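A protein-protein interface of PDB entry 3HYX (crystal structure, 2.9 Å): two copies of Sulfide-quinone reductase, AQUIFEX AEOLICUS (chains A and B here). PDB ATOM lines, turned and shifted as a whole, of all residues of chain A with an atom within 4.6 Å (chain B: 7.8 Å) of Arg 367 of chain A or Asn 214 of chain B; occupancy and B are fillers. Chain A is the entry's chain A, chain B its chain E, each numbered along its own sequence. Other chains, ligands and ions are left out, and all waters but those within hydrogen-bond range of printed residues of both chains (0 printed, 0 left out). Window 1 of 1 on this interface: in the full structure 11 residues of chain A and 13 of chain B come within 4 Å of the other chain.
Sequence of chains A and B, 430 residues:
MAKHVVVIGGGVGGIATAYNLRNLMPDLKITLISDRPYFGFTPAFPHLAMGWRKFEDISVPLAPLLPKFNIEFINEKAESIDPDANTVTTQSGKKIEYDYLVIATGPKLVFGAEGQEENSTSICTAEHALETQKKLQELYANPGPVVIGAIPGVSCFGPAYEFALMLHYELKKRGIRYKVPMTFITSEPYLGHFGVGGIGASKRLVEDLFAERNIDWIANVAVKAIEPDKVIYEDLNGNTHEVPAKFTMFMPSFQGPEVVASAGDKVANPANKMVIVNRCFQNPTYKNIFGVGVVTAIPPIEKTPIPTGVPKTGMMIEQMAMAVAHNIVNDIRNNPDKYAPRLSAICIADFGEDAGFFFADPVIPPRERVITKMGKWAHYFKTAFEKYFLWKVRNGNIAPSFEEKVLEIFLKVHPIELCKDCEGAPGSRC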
ATOM      1  N   VAL A 196     -26.729 -20.426  40.707  1.00  0.00           N
ATOM      2  CA  VAL A 196     -26.513 -19.598  39.525  1.00  0.00           C
ATOM      3  C   VAL A 196     -26.245 -20.416  38.266  1.00  0.00           C
ATOM      4  O   VAL A 196     -25.792 -19.871  37.253  1.00  0.00           O
ATOM      5  CB  VAL A 196     -25.354 -18.582  39.737  1.00  0.00           C
ATOM      6  CG1 VAL A 196     -25.580 -17.748  41.012  1.00  0.00           C
ATOM      7  CG2 VAL A 196     -23.988 -19.282  39.787  1.00  0.00           C
ATOM      8  N   GLY A 198     -23.959 -22.666  37.966  1.00  0.00           N
ATOM      9  CA  GLY A 198     -22.518 -22.777  37.783  1.00  0.00           C
ATOM     10  C   GLY A 198     -21.847 -21.467  37.434  1.00  0.00           C
ATOM     11  O   GLY A 198     -22.484 -20.545  36.932  1.00  0.00           O
ATOM     12  N   ILE A 199     -20.562 -21.380  37.752  1.00  0.00           N
ATOM     13  CA  ILE A 199     -19.716 -20.272  37.346  1.00  0.00           C
ATOM     14  C   ILE A 199     -18.560 -20.927  36.619  1.00  0.00           C
ATOM     15  O   ILE A 199     -17.695 -21.525  37.244  1.00  0.00           O
ATOM     16  CB  ILE A 199     -19.220 -19.438  38.542  1.00  0.00           C
ATOM     17  CG1 ILE A 199     -20.410 -18.813  39.286  1.00  0.00           C
ATOM     18  CG2 ILE A 199     -18.267 -18.351  38.071  1.00  0.00           C
ATOM     19  CD1 ILE A 199     -20.080 -18.214  40.670  1.00  0.00           C
ATOM     20  N   GLY A 200     -18.576 -20.856  35.290  1.00  0.00           N
ATOM     21  CA  GLY A 200     -17.587 -21.557  34.474  1.00  0.00           C
ATOM     22  C   GLY A 200     -17.596 -23.043  34.754  1.00  0.00           C
ATOM     23  O   GLY A 200     -18.658 -23.663  34.789  1.00  0.00           O
ATOM     24  N   ALA A 360     -17.941 -13.773  38.034  1.00  0.00           N
ATOM     25  CA  ALA A 360     -19.017 -13.882  37.046  1.00  0.00           C
ATOM     26  C   ALA A 360     -19.517 -12.506  36.656  1.00  0.00           C
ATOM     27  O   ALA A 360     -19.870 -11.703  37.517  1.00  0.00           O
ATOM     28  CB  ALA A 360     -20.156 -14.722  37.575  1.00  0.00           C
ATOM     29  N   ASP A 361     -19.542 -12.245  35.352  1.00  0.00           N
ATOM     30  CA  ASP A 361     -19.966 -10.954  34.830  1.00  0.00           C
ATOM     31  C   ASP A 361     -20.990 -11.035  33.678  1.00  0.00           C
ATOM     32  O   ASP A 361     -20.609 -11.298  32.528  1.00  0.00           O
ATOM     33  CB  ASP A 361     -18.745 -10.168  34.368  1.00  0.00           C
ATOM     34  CG  ASP A 361     -19.098  -8.777  33.890  1.00  0.00           C
ATOM     35  OD1 ASP A 361     -20.033  -8.181  34.491  1.00  0.00           O
ATOM     36  OD2 ASP A 361     -18.448  -8.291  32.923  1.00  0.00           O
ATOM     37  N   PRO A 362     -22.288 -10.793  33.977  1.00  0.00           N
ATOM     38  CA  PRO A 362     -22.876 -10.627  35.298  1.00  0.00           C
ATOM     39  C   PRO A 362     -23.079 -11.991  35.936  1.00  0.00           C
ATOM     40  O   PRO A 362     -22.620 -12.978  35.379  1.00  0.00           O
ATOM     41  CB  PRO A 362     -24.234  -9.972  34.996  1.00  0.00           C
ATOM     42  CG  PRO A 362     -24.195  -9.586  33.543  1.00  0.00           C
ATOM     43  CD  PRO A 362     -23.302 -10.595  32.929  1.00  0.00           C
ATOM     44  N   VAL A 363     -23.749 -12.043  37.087  1.00  0.00           N
ATOM     45  CA  VAL A 363     -24.108 -13.313  37.731  1.00  0.00           C
ATOM     46  C   VAL A 363     -25.305 -14.012  37.039  1.00  0.00           C
ATOM     47  O   VAL A 363     -25.315 -15.242  36.877  1.00  0.00           O
ATOM     48  CB  VAL A 363     -24.404 -13.110  39.242  1.00  0.00           C
ATOM     49  CG1 VAL A 363     -24.825 -14.402  39.893  1.00  0.00           C
ATOM     50  CG2 VAL A 363     -23.175 -12.565  39.934  1.00  0.00           C
ATOM     51  N   PRO A 365     -27.236 -15.119  33.923  1.00  0.00           N
ATOM     52  CA  PRO A 365     -26.850 -15.355  32.537  1.00  0.00           C
ATOM     53  C   PRO A 365     -27.795 -14.664  31.562  1.00  0.00           C
ATOM     54  O   PRO A 365     -28.940 -14.379  31.923  1.00  0.00           O
ATOM     55  CB  PRO A 365     -26.937 -16.876  32.404  1.00  0.00           C
ATOM     56  CG  PRO A 365     -26.868 -17.392  33.786  1.00  0.00           C
ATOM     57  CD  PRO A 365     -27.606 -16.378  34.586  1.00  0.00           C
ATOM     58  N   PRO A 366     -27.324 -14.398  30.332  1.00  0.00           N
ATOM     59  CA  PRO A 366     -26.013 -14.820  29.819  1.00  0.00           C
ATOM     60  C   PRO A 366     -24.825 -13.935  30.246  1.00  0.00           C
ATOM     61  O   PRO A 366     -24.930 -12.706  30.258  1.00  0.00           O
ATOM     62  CB  PRO A 366     -26.200 -14.789  28.299  1.00  0.00           C
ATOM     63  CG  PRO A 366     -27.286 -13.797  28.069  1.00  0.00           C
ATOM     64  CD  PRO A 366     -28.089 -13.631  29.336  1.00  0.00           C
ATOM     65  N   ARG A 367     -23.707 -14.584  30.572  1.00  0.00           N
ATOM     66  CA  ARG A 367     -22.505 -13.917  31.052  1.00  0.00           C
ATOM     67  C   ARG A 367     -21.556 -13.480  29.946  1.00  0.00           C
ATOM     68  O   ARG A 367     -21.409 -14.166  28.935  1.00  0.00           O
ATOM     69  CB  ARG A 367     -21.767 -14.844  32.004  1.00  0.00           C
ATOM     70  CG  ARG A 367     -22.668 -15.458  33.028  1.00  0.00           C
ATOM     71  CD  ARG A 367     -21.908 -15.827  34.257  1.00  0.00           C
ATOM     72  NE  ARG A 367     -22.804 -16.241  35.332  1.00  0.00           N
ATOM     73  CZ  ARG A 367     -22.914 -17.485  35.773  1.00  0.00           C
ATOM     74  NH1 ARG A 367     -23.749 -17.761  36.759  1.00  0.00           N
ATOM     75  NH2 ARG A 367     -22.184 -18.448  35.237  1.00  0.00           N
ATOM     76  N   GLU A 368     -20.907 -12.334  30.159  1.00  0.00           N
ATOM     77  CA  GLU A 368     -19.879 -11.810  29.245  1.00  0.00           C
ATOM     78  C   GLU A 368     -18.587 -12.618  29.395  1.00  0.00           C
ATOM     79  O   GLU A 368     -17.957 -12.985  28.392  1.00  0.00           O
ATOM     80  CB  GLU A 368     -19.608 -10.330  29.536  1.00  0.00           C
ATOM     81  CG  GLU A 368     -18.818  -9.601  28.472  1.00  0.00           C
ATOM     82  CD  GLU A 368     -19.689  -9.079  27.325  1.00  0.00           C
ATOM     83  OE1 GLU A 368     -20.910  -8.882  27.544  1.00  0.00           O
ATOM     84  OE2 GLU A 368     -19.149  -8.853  26.208  1.00  0.00           O
ATOM     85  N   ARG A 369     -18.206 -12.876  30.653  1.00  0.00           N
ATOM     86  CA  ARG A 369     -17.041 -13.691  30.981  1.00  0.00           C
ATOM     87  C   ARG A 369     -17.078 -14.200  32.401  1.00  0.00           C
ATOM     88  O   ARG A 369     -17.782 -13.653  33.248  1.00  0.00           O
ATOM     89  CB  ARG A 369     -15.736 -12.928  30.738  1.00  0.00           C
ATOM     90  CG  ARG A 369     -15.322 -11.931  31.807  1.00  0.00           C
ATOM     91  CD  ARG A 369     -14.042 -11.184  31.385  1.00  0.00           C
ATOM     92  NE  ARG A 369     -14.239 -10.403  30.155  1.00  0.00           N
ATOM     93  CZ  ARG A 369     -14.859  -9.218  30.095  1.00  0.00           C
ATOM     94  NH1 ARG A 369     -15.351  -8.648  31.202  1.00  0.00           N
ATOM     95  NH2 ARG A 369     -14.988  -8.604  28.920  1.00  0.00           N
ATOM     96  N   VAL A 370     -16.322 -15.268  32.648  1.00  0.00           N
ATOM     97  CA  VAL A 370     -16.138 -15.798  34.006  1.00  0.00           C
ATOM     98  C   VAL A 370     -14.665 -16.072  34.272  1.00  0.00           C
ATOM     99  O   VAL A 370     -13.881 -16.223  33.346  1.00  0.00           O
ATOM    100  CB  VAL A 370     -16.961 -17.097  34.306  1.00  0.00           C
ATOM    101  CG1 VAL A 370     -18.442 -16.874  34.107  1.00  0.00           C
ATOM    102  CG2 VAL A 370     -16.479 -18.257  33.471  1.00  0.00           C
ATOM    103  N   LEU B 165     -18.575 -21.517  18.821  1.00  0.00           N
ATOM    104  CA  LEU B 165     -17.460 -20.860  19.491  1.00  0.00           C
ATOM    105  C   LEU B 165     -17.067 -19.515  18.872  1.00  0.00           C
ATOM    106  O   LEU B 165     -16.965 -18.505  19.575  1.00  0.00           O
ATOM    107  CB  LEU B 165     -16.244 -21.800  19.614  1.00  0.00           C
ATOM    108  CG  LEU B 165     -16.069 -22.639  20.896  1.00  0.00           C
ATOM    109  CD1 LEU B 165     -16.425 -21.839  22.164  1.00  0.00           C
ATOM    110  CD2 LEU B 165     -16.861 -23.930  20.853  1.00  0.00           C
ATOM    111  N   HIS B 168     -19.568 -16.846  19.587  1.00  0.00           N
ATOM    112  CA  HIS B 168     -19.404 -16.381  20.960  1.00  0.00           C
ATOM    113  C   HIS B 168     -18.316 -15.306  21.026  1.00  0.00           C
ATOM    114  O   HIS B 168     -18.499 -14.252  21.644  1.00  0.00           O
ATOM    115  CB  HIS B 168     -19.083 -17.548  21.896  1.00  0.00           C
ATOM    116  CG  HIS B 168     -18.493 -17.126  23.203  1.00  0.00           C
ATOM    117  ND1 HIS B 168     -19.262 -16.683  24.256  1.00  0.00           N
ATOM    118  CD2 HIS B 168     -17.208 -17.067  23.625  1.00  0.00           C
ATOM    119  CE1 HIS B 168     -18.477 -16.373  25.272  1.00  0.00           C
ATOM    120  NE2 HIS B 168     -17.225 -16.595  24.914  1.00  0.00           N
ATOM    121  N   LYS B 172     -18.962 -11.237  22.030  1.00  0.00           N
ATOM    122  CA  LYS B 172     -18.111 -10.659  23.050  1.00  0.00           C
ATOM    123  C   LYS B 172     -17.386  -9.415  22.512  1.00  0.00           C
ATOM    124  O   LYS B 172     -17.345  -8.393  23.189  1.00  0.00           O
ATOM    125  CB  LYS B 172     -17.118 -11.718  23.534  1.00  0.00           C
ATOM    126  CG  LYS B 172     -17.097 -11.927  25.028  1.00  0.00           C
ATOM    127  CD  LYS B 172     -16.163 -13.065  25.362  1.00  0.00           C
ATOM    128  CE  LYS B 172     -15.376 -12.774  26.633  1.00  0.00           C
ATOM    129  NZ  LYS B 172     -14.020 -13.394  26.564  1.00  0.00           N
ATOM    130  N   ILE B 176     -22.018  -7.479  23.187  1.00  0.00           N
ATOM    131  CA  ILE B 176     -23.440  -7.822  23.307  1.00  0.00           C
ATOM    132  C   ILE B 176     -23.688  -9.267  23.762  1.00  0.00           C
ATOM    133  O   ILE B 176     -24.832  -9.743  23.753  1.00  0.00           O
ATOM    134  CB  ILE B 176     -24.259  -7.496  22.018  1.00  0.00           C
ATOM    135  CG1 ILE B 176     -23.665  -8.191  20.791  1.00  0.00           C
ATOM    136  CG2 ILE B 176     -24.378  -5.990  21.819  1.00  0.00           C
ATOM    137  CD1 ILE B 176     -24.720  -8.715  19.832  1.00  0.00           C
ATOM    138  N   ARG B 177     -22.622  -9.949  24.174  1.00  0.00           N
ATOM    139  CA  ARG B 177     -22.714 -11.350  24.587  1.00  0.00           C
ATOM    140  C   ARG B 177     -23.737 -11.545  25.693  1.00  0.00           C
ATOM    141  O   ARG B 177     -24.492 -12.514  25.675  1.00  0.00           O
ATOM    142  CB  ARG B 177     -21.348 -11.876  25.033  1.00  0.00           C
ATOM    143  CG  ARG B 177     -21.310 -13.320  25.552  1.00  0.00           C
ATOM    144  CD  ARG B 177     -21.754 -14.320  24.514  1.00  0.00           C
ATOM    145  NE  ARG B 177     -23.007 -14.954  24.905  1.00  0.00           N
ATOM    146  CZ  ARG B 177     -23.129 -16.235  25.256  1.00  0.00           C
ATOM    147  NH1 ARG B 177     -22.076 -17.051  25.259  1.00  0.00           N
ATOM    148  NH2 ARG B 177     -24.318 -16.704  25.607  1.00  0.00           N
ATOM    149  N   TYR B 178     -23.771 -10.613  26.636  1.00  0.00           N
ATOM    150  CA  TYR B 178     -24.631 -10.723  27.803  1.00  0.00           C
ATOM    151  C   TYR B 178     -26.107 -10.390  27.501  1.00  0.00           C
ATOM    152  O   TYR B 178     -26.951 -10.346  28.415  1.00  0.00           O
ATOM    153  CB  TYR B 178     -24.081  -9.830  28.916  1.00  0.00           C
ATOM    154  CG  TYR B 178     -24.522  -8.387  28.831  1.00  0.00           C
ATOM    155  CD1 TYR B 178     -25.279  -7.817  29.851  1.00  0.00           C
ATOM    156  CD2 TYR B 178     -24.193  -7.594  27.731  1.00  0.00           C
ATOM    157  CE1 TYR B 178     -25.692  -6.492  29.791  1.00  0.00           C
ATOM    158  CE2 TYR B 178     -24.608  -6.268  27.655  1.00  0.00           C
ATOM    159  CZ  TYR B 178     -25.354  -5.725  28.689  1.00  0.00           C
ATOM    160  OH  TYR B 178     -25.765  -4.414  28.631  1.00  0.00           O
ATOM    161  N   LYS B 179     -26.404 -10.142  26.223  1.00  0.00           N
ATOM    162  CA  LYS B 179     -27.766  -9.844  25.765  1.00  0.00           C
ATOM    163  C   LYS B 179     -28.254 -10.992  24.902  1.00  0.00           C
ATOM    164  O   LYS B 179     -29.392 -10.998  24.435  1.00  0.00           O
ATOM    165  CB  LYS B 179     -27.795  -8.548  24.940  1.00  0.00           C
ATOM    166  CG  LYS B 179     -27.664  -7.255  25.725  1.00  0.00           C
ATOM    167  CD  LYS B 179     -29.034  -6.639  26.008  1.00  0.00           C
ATOM    168  CE  LYS B 179     -28.948  -5.131  26.188  1.00  0.00           C
ATOM    169  NZ  LYS B 179     -28.284  -4.483  25.011  1.00  0.00           N
ATOM    170  N   VAL B 180     -27.374 -11.966  24.693  1.00  0.00           N
ATOM    171  CA  VAL B 180     -27.629 -13.066  23.766  1.00  0.00           C
ATOM    172  C   VAL B 180     -27.317 -14.428  24.393  1.00  0.00           C
ATOM    173  O   VAL B 180     -26.147 -14.816  24.447  1.00  0.00           O
ATOM    174  CB  VAL B 180     -26.792 -12.904  22.479  1.00  0.00           C
ATOM    175  CG1 VAL B 180     -27.185 -13.937  21.459  1.00  0.00           C
ATOM    176  CG2 VAL B 180     -26.953 -11.509  21.905  1.00  0.00           C
ATOM    177  N   PRO B 181     -28.356 -15.152  24.880  1.00  0.00           N
ATOM    178  CA  PRO B 181     -28.180 -16.542  25.323  1.00  0.00           C
ATOM    179  C   PRO B 181     -27.661 -17.403  24.177  1.00  0.00           C
ATOM    180  O   PRO B 181     -27.812 -17.027  23.015  1.00  0.00           O
ATOM    181  CB  PRO B 181     -29.602 -16.982  25.688  1.00  0.00           C
ATOM    182  CG  PRO B 181     -30.336 -15.735  25.964  1.00  0.00           C
ATOM    183  CD  PRO B 181     -29.750 -14.701  25.057  1.00  0.00           C
ATOM    184  N   MET B 182     -27.038 -18.534  24.500  1.00  0.00           N
ATOM    185  CA  MET B 182     -26.617 -19.510  23.485  1.00  0.00           C
ATOM    186  C   MET B 182     -26.900 -20.945  23.922  1.00  0.00           C
ATOM    187  O   MET B 182     -26.584 -21.326  25.049  1.00  0.00           O
ATOM    188  CB  MET B 182     -25.135 -19.355  23.152  1.00  0.00           C
ATOM    189  CG  MET B 182     -24.779 -18.026  22.522  1.00  0.00           C
ATOM    190  SD  MET B 182     -23.082 -17.955  21.951  1.00  0.00           S
ATOM    191  CE  MET B 182     -23.220 -18.771  20.354  1.00  0.00           C
ATOM    192  N   THR B 183     -27.505 -21.732  23.034  1.00  0.00           N
ATOM    193  CA  THR B 183     -27.672 -23.161  23.284  1.00  0.00           C
ATOM    194  C   THR B 183     -27.244 -24.030  22.109  1.00  0.00           C
ATOM    195  O   THR B 183     -27.677 -23.808  20.980  1.00  0.00           O
ATOM    196  CB  THR B 183     -29.101 -23.514  23.657  1.00  0.00           C
ATOM    197  OG1 THR B 183     -29.675 -22.441  24.409  1.00  0.00           O
ATOM    198  CG2 THR B 183     -29.115 -24.781  24.497  1.00  0.00           C
ATOM    199  N   GLU B 207     -16.868 -29.796  27.094  1.00  0.00           N
ATOM    200  CA  GLU B 207     -17.812 -29.470  28.127  1.00  0.00           C
ATOM    201  C   GLU B 207     -17.271 -28.292  28.890  1.00  0.00           C
ATOM    202  O   GLU B 207     -17.980 -27.304  29.069  1.00  0.00           O
ATOM    203  CB  GLU B 207     -18.036 -30.659  29.051  1.00  0.00           C
ATOM    204  CG  GLU B 207     -18.930 -31.731  28.452  1.00  0.00           C
ATOM    205  CD  GLU B 207     -19.287 -32.817  29.446  1.00  0.00           C
ATOM    206  OE1 GLU B 207     -18.718 -32.819  30.559  1.00  0.00           O
ATOM    207  OE2 GLU B 207     -20.140 -33.670  29.111  1.00  0.00           O
ATOM    208  N   ASP B 208     -16.006 -28.395  29.302  1.00  0.00           N
ATOM    209  CA  ASP B 208     -15.320 -27.332  30.037  1.00  0.00           C
ATOM    210  C   ASP B 208     -15.220 -26.059  29.225  1.00  0.00           C
ATOM    211  O   ASP B 208     -15.313 -24.962  29.768  1.00  0.00           O
ATOM    212  CB  ASP B 208     -13.921 -27.773  30.474  1.00  0.00           C
ATOM    213  CG  ASP B 208     -13.945 -28.712  31.675  1.00  0.00           C
ATOM    214  OD1 ASP B 208     -14.993 -28.812  32.355  1.00  0.00           O
ATOM    215  OD2 ASP B 208     -12.904 -29.349  31.941  1.00  0.00           O
ATOM    216  N   LEU B 209     -15.038 -26.216  27.921  1.00  0.00           N
ATOM    217  CA  LEU B 209     -14.981 -25.090  27.003  1.00  0.00           C
ATOM    218  C   LEU B 209     -16.305 -24.319  26.988  1.00  0.00           C
ATOM    219  O   LEU B 209     -16.325 -23.082  26.982  1.00  0.00           O
ATOM    220  CB  LEU B 209     -14.641 -25.596  25.608  1.00  0.00           C
ATOM    221  CG  LEU B 209     -14.172 -24.598  24.562  1.00  0.00           C
ATOM    222  CD1 LEU B 209     -12.969 -23.802  25.049  1.00  0.00           C
ATOM    223  CD2 LEU B 209     -13.831 -25.377  23.306  1.00  0.00           C
ATOM    224  N   PHE B 210     -17.407 -25.060  27.020  1.00  0.00           N
ATOM    225  CA  PHE B 210     -18.731 -24.478  26.963  1.00  0.00           C
ATOM    226  C   PHE B 210     -19.116 -23.822  28.267  1.00  0.00           C
ATOM    227  O   PHE B 210     -19.934 -22.901  28.293  1.00  0.00           O
ATOM    228  CB  PHE B 210     -19.745 -25.556  26.594  1.00  0.00           C
ATOM    229  CG  PHE B 210     -19.908 -25.743  25.118  1.00  0.00           C
ATOM    230  CD1 PHE B 210     -18.876 -25.426  24.245  1.00  0.00           C
ATOM    231  CD2 PHE B 210     -21.090 -26.245  24.603  1.00  0.00           C
ATOM    232  CE1 PHE B 210     -19.027 -25.595  22.901  1.00  0.00           C
ATOM    233  CE2 PHE B 210     -21.252 -26.422  23.246  1.00  0.00           C
ATOM    234  CZ  PHE B 210     -20.222 -26.097  22.392  1.00  0.00           C
ATOM    235  N   ALA B 211     -18.526 -24.300  29.352  1.00  0.00           N
ATOM    236  CA  ALA B 211     -18.846 -23.782  30.666  1.00  0.00           C
ATOM    237  C   ALA B 211     -18.215 -22.406  30.859  1.00  0.00           C
ATOM    238  O   ALA B 211     -18.905 -21.467  31.246  1.00  0.00           O
ATOM    239  CB  ALA B 211     -18.410 -24.760  31.749  1.00  0.00           C
ATOM    240  N   GLU B 212     -16.921 -22.289  30.558  1.00  0.00           N
ATOM    241  CA  GLU B 212     -16.198 -21.015  30.679  1.00  0.00           C
ATOM    242  C   GLU B 212     -16.870 -19.929  29.864  1.00  0.00           C
ATOM    243  O   GLU B 212     -16.917 -18.769  30.279  1.00  0.00           O
ATOM    244  CB  GLU B 212     -14.750 -21.154  30.200  1.00  0.00           C
ATOM    245  CG  GLU B 212     -13.780 -21.746  31.214  1.00  0.00           C
ATOM    246  CD  GLU B 212     -12.874 -22.828  30.603  1.00  0.00           C
ATOM    247  OE1 GLU B 212     -12.452 -22.708  29.416  1.00  0.00           O
ATOM    248  OE2 GLU B 212     -12.596 -23.816  31.325  1.00  0.00           O
ATOM    249  N   ARG B 213     -17.394 -20.327  28.707  1.00  0.00           N
ATOM    250  CA  ARG B 213     -17.925 -19.390  27.730  1.00  0.00           C
ATOM    251  C   ARG B 213     -19.446 -19.252  27.767  1.00  0.00           C
ATOM    252  O   ARG B 213     -20.023 -18.456  27.023  1.00  0.00           O
ATOM    253  CB  ARG B 213     -17.396 -19.742  26.342  1.00  0.00           C
ATOM    254  CG  ARG B 213     -15.909 -19.460  26.258  1.00  0.00           C
ATOM    255  CD  ARG B 213     -15.194 -20.178  25.143  1.00  0.00           C
ATOM    256  NE  ARG B 213     -13.744 -20.077  25.334  1.00  0.00           N
ATOM    257  CZ  ARG B 213     -12.838 -20.296  24.386  1.00  0.00           C
ATOM    258  NH1 ARG B 213     -13.209 -20.636  23.155  1.00  0.00           N
ATOM    259  NH2 ARG B 213     -11.549 -20.179  24.665  1.00  0.00           N
ATOM    260  N   ASN B 214     -20.087 -20.009  28.655  1.00  0.00           N
ATOM    261  CA  ASN B 214     -21.515 -19.855  28.929  1.00  0.00           C
ATOM    262  C   ASN B 214     -22.416 -20.303  27.783  1.00  0.00           C
ATOM    263  O   ASN B 214     -23.518 -19.777  27.598  1.00  0.00           O
ATOM    264  CB  ASN B 214     -21.831 -18.412  29.329  1.00  0.00           C
ATOM    265  CG  ASN B 214     -23.141 -18.288  30.055  1.00  0.00           C
ATOM    266  OD1 ASN B 214     -23.477 -19.123  30.886  1.00  0.00           O
ATOM    267  ND2 ASN B 214     -23.897 -17.248  29.740  1.00  0.00           N
ATOM    268  N   ILE B 215     -21.942 -21.280  27.021  1.00  0.00           N
ATOM    269  CA  ILE B 215     -22.767 -21.911  26.004  1.00  0.00           C
ATOM    270  C   ILE B 215     -23.497 -23.110  26.614  1.00  0.00           C
ATOM    271  O   ILE B 215     -22.883 -24.143  26.892  1.00  0.00           O
ATOM    272  CB  ILE B 215     -21.936 -22.339  24.778  1.00  0.00           C
ATOM    273  CG1 ILE B 215     -21.243 -21.117  24.159  1.00  0.00           C
ATOM    274  CG2 ILE B 215     -22.816 -23.056  23.759  1.00  0.00           C
ATOM    275  CD1 ILE B 215     -20.151 -21.444  23.137  1.00  0.00           C
ATOM    276  N   ASP B 216     -24.801 -22.952  26.843  1.00  0.00           N
ATOM    277  CA  ASP B 216     -25.643 -24.035  27.345  1.00  0.00           C
ATOM    278  C   ASP B 216     -25.741 -25.092  26.269  1.00  0.00           C
ATOM    279  O   ASP B 216     -25.469 -24.815  25.102  1.00  0.00           O
ATOM    280  CB  ASP B 216     -27.042 -23.522  27.683  1.00  0.00           C
ATOM    281  CG  ASP B 216     -27.035 -22.437  28.754  1.00  0.00           C
ATOM    282  OD1 ASP B 216     -26.123 -22.415  29.615  1.00  0.00           O
ATOM    283  OD2 ASP B 216     -27.963 -21.599  28.743  1.00  0.00           O
ATOM    284  N   TRP B 217     -26.119 -26.305  26.655  1.00  0.00           N
ATOM    285  CA  TRP B 217     -26.203 -27.405  25.700  1.00  0.00           C
ATOM    286  C   TRP B 217     -27.226 -28.477  26.073  1.00  0.00           C
ATOM    287  O   TRP B 217     -27.526 -28.679  27.242  1.00  0.00           O
ATOM    288  CB  TRP B 217     -24.814 -28.024  25.464  1.00  0.00           C
ATOM    289  CG  TRP B 217     -24.082 -28.386  26.726  1.00  0.00           C
ATOM    290  CD1 TRP B 217     -23.256 -27.578  27.472  1.00  0.00           C
ATOM    291  CD2 TRP B 217     -24.110 -29.650  27.389  1.00  0.00           C
ATOM    292  NE1 TRP B 217     -22.774 -28.268  28.557  1.00  0.00           N
ATOM    293  CE2 TRP B 217     -23.280 -29.543  28.530  1.00  0.00           C
ATOM    294  CE3 TRP B 217     -24.758 -30.867  27.132  1.00  0.00           C
ATOM    295  CZ2 TRP B 217     -23.082 -30.609  29.413  1.00  0.00           C
ATOM    296  CZ3 TRP B 217     -24.559 -31.930  28.005  1.00  0.00           C
ATOM    297  CH2 TRP B 217     -23.732 -31.793  29.133  1.00  0.00           C
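Along chain A the printed residues that touch a printed residue of chain B span positions 200 to 370. Printed residues of chain B that touch a printed residue of chain A: Lys 172, Arg 177, Tyr 178, Val 180, Pro 181, Ala 211, Glu 212 and Asn 214. Among the printed residues, no Asp or Glu carboxylate lies within 4 Å of a Lys or Arg side-chain nitrogen of the other chain.
Ile 199 of chain A touches none of the printed residues of chain B. Of chain B, only Arg 177 (3.5 Å) and Asn 214 (2.8 Å) come within 4 Å of Arg 367 of chain A. Of the printed residues of chain B, Val 370 of chain A touches Glu 212. Of the printed residues of chain A, Arg 177 of chain B touches Pro 366, Arg 367 and Glu 368. Printed residues of chain A within 4 Å of Pro 181 of chain B: Pro 366 (3.6 Å). Asn 214 of chain B touches just these residues of chain A: Pro 366 and Arg 367. The nearest residue of chain B that does not touch Arg 367 of chain A is Tyr 178 of chain B (4.6 Å). The nearest residue of chain A that does not touch Asn 214 of chain B is Pro 365 of chain A (4.1 Å). The nearest printed residue of chain A that does not touch Val 180 of chain B is Arg 367 of chain A (6.6 Å).
No position is printed for both chains.
ND2 of Asn 214 of chain B lies close to N of Arg 367 of chain A (2.8 Å). The backbone NH (N) of Tyr 178 of chain B sits at hydrogen-bond distance from the side-chain carboxylate (OE1) of Glu 368 of chain A.
Among the printed residues, pairs that only touch across the chains: Glu 368 of chain A with Lys 172 of chain B (3.1 Å), Pro 366 of chain A with Tyr 178 of chain B (3.2 Å), Pro 366 of chain A with Asn 214 of chain B (3.2 Å), Gly 200 of chain A with Ala 211 of chain B (3.2 Å), Val 370 of chain A with Glu 212 of chain B (3.3 Å), Arg 367 of chain A with Arg 177 of chain B (3.5 Å), Pro 366 of chain A with Pro 181 of chain B (3.6 Å), Pro 366 of chain A with Val 180 of chain B (3.7 Å), Pro 366 of chain A with Arg 177 of chain B (3.8 Å) and Glu 368 of chain A with Arg 177 of chain B (3.9 Å).
The guanidinium group (NH1) of Arg 367 of chain A is in hydrogen-bond range of the backbone carbonyl oxygen (O) of Val 196 of chain A (3.0 Å). The backbone carbonyl oxygen of Gly 198 of chain A sits at hydrogen-bond distance from the guanidinium group of Arg 367 of chain A (2.7 Å). The backbone carbonyl oxygen of Val 363 of chain A lies within hydrogen-bond range of the guanidinium group of Arg 367 of chain A (3.0 Å). A ring nitrogen (ND1) of His 168 of chain B lies within hydrogen-bond range of the guanidinium group (NH1) of Arg 177 of chain B (3.0 Å). NH1 of Arg 177 of chain B lies within hydrogen-bond range of SD of Met 182 of chain B, at 3.6 Å. The guanidinium group (NH1) of Arg 177 of chain B sits at hydrogen-bond distance from the backbone carbonyl oxygen (O) of Arg 213 of chain B.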
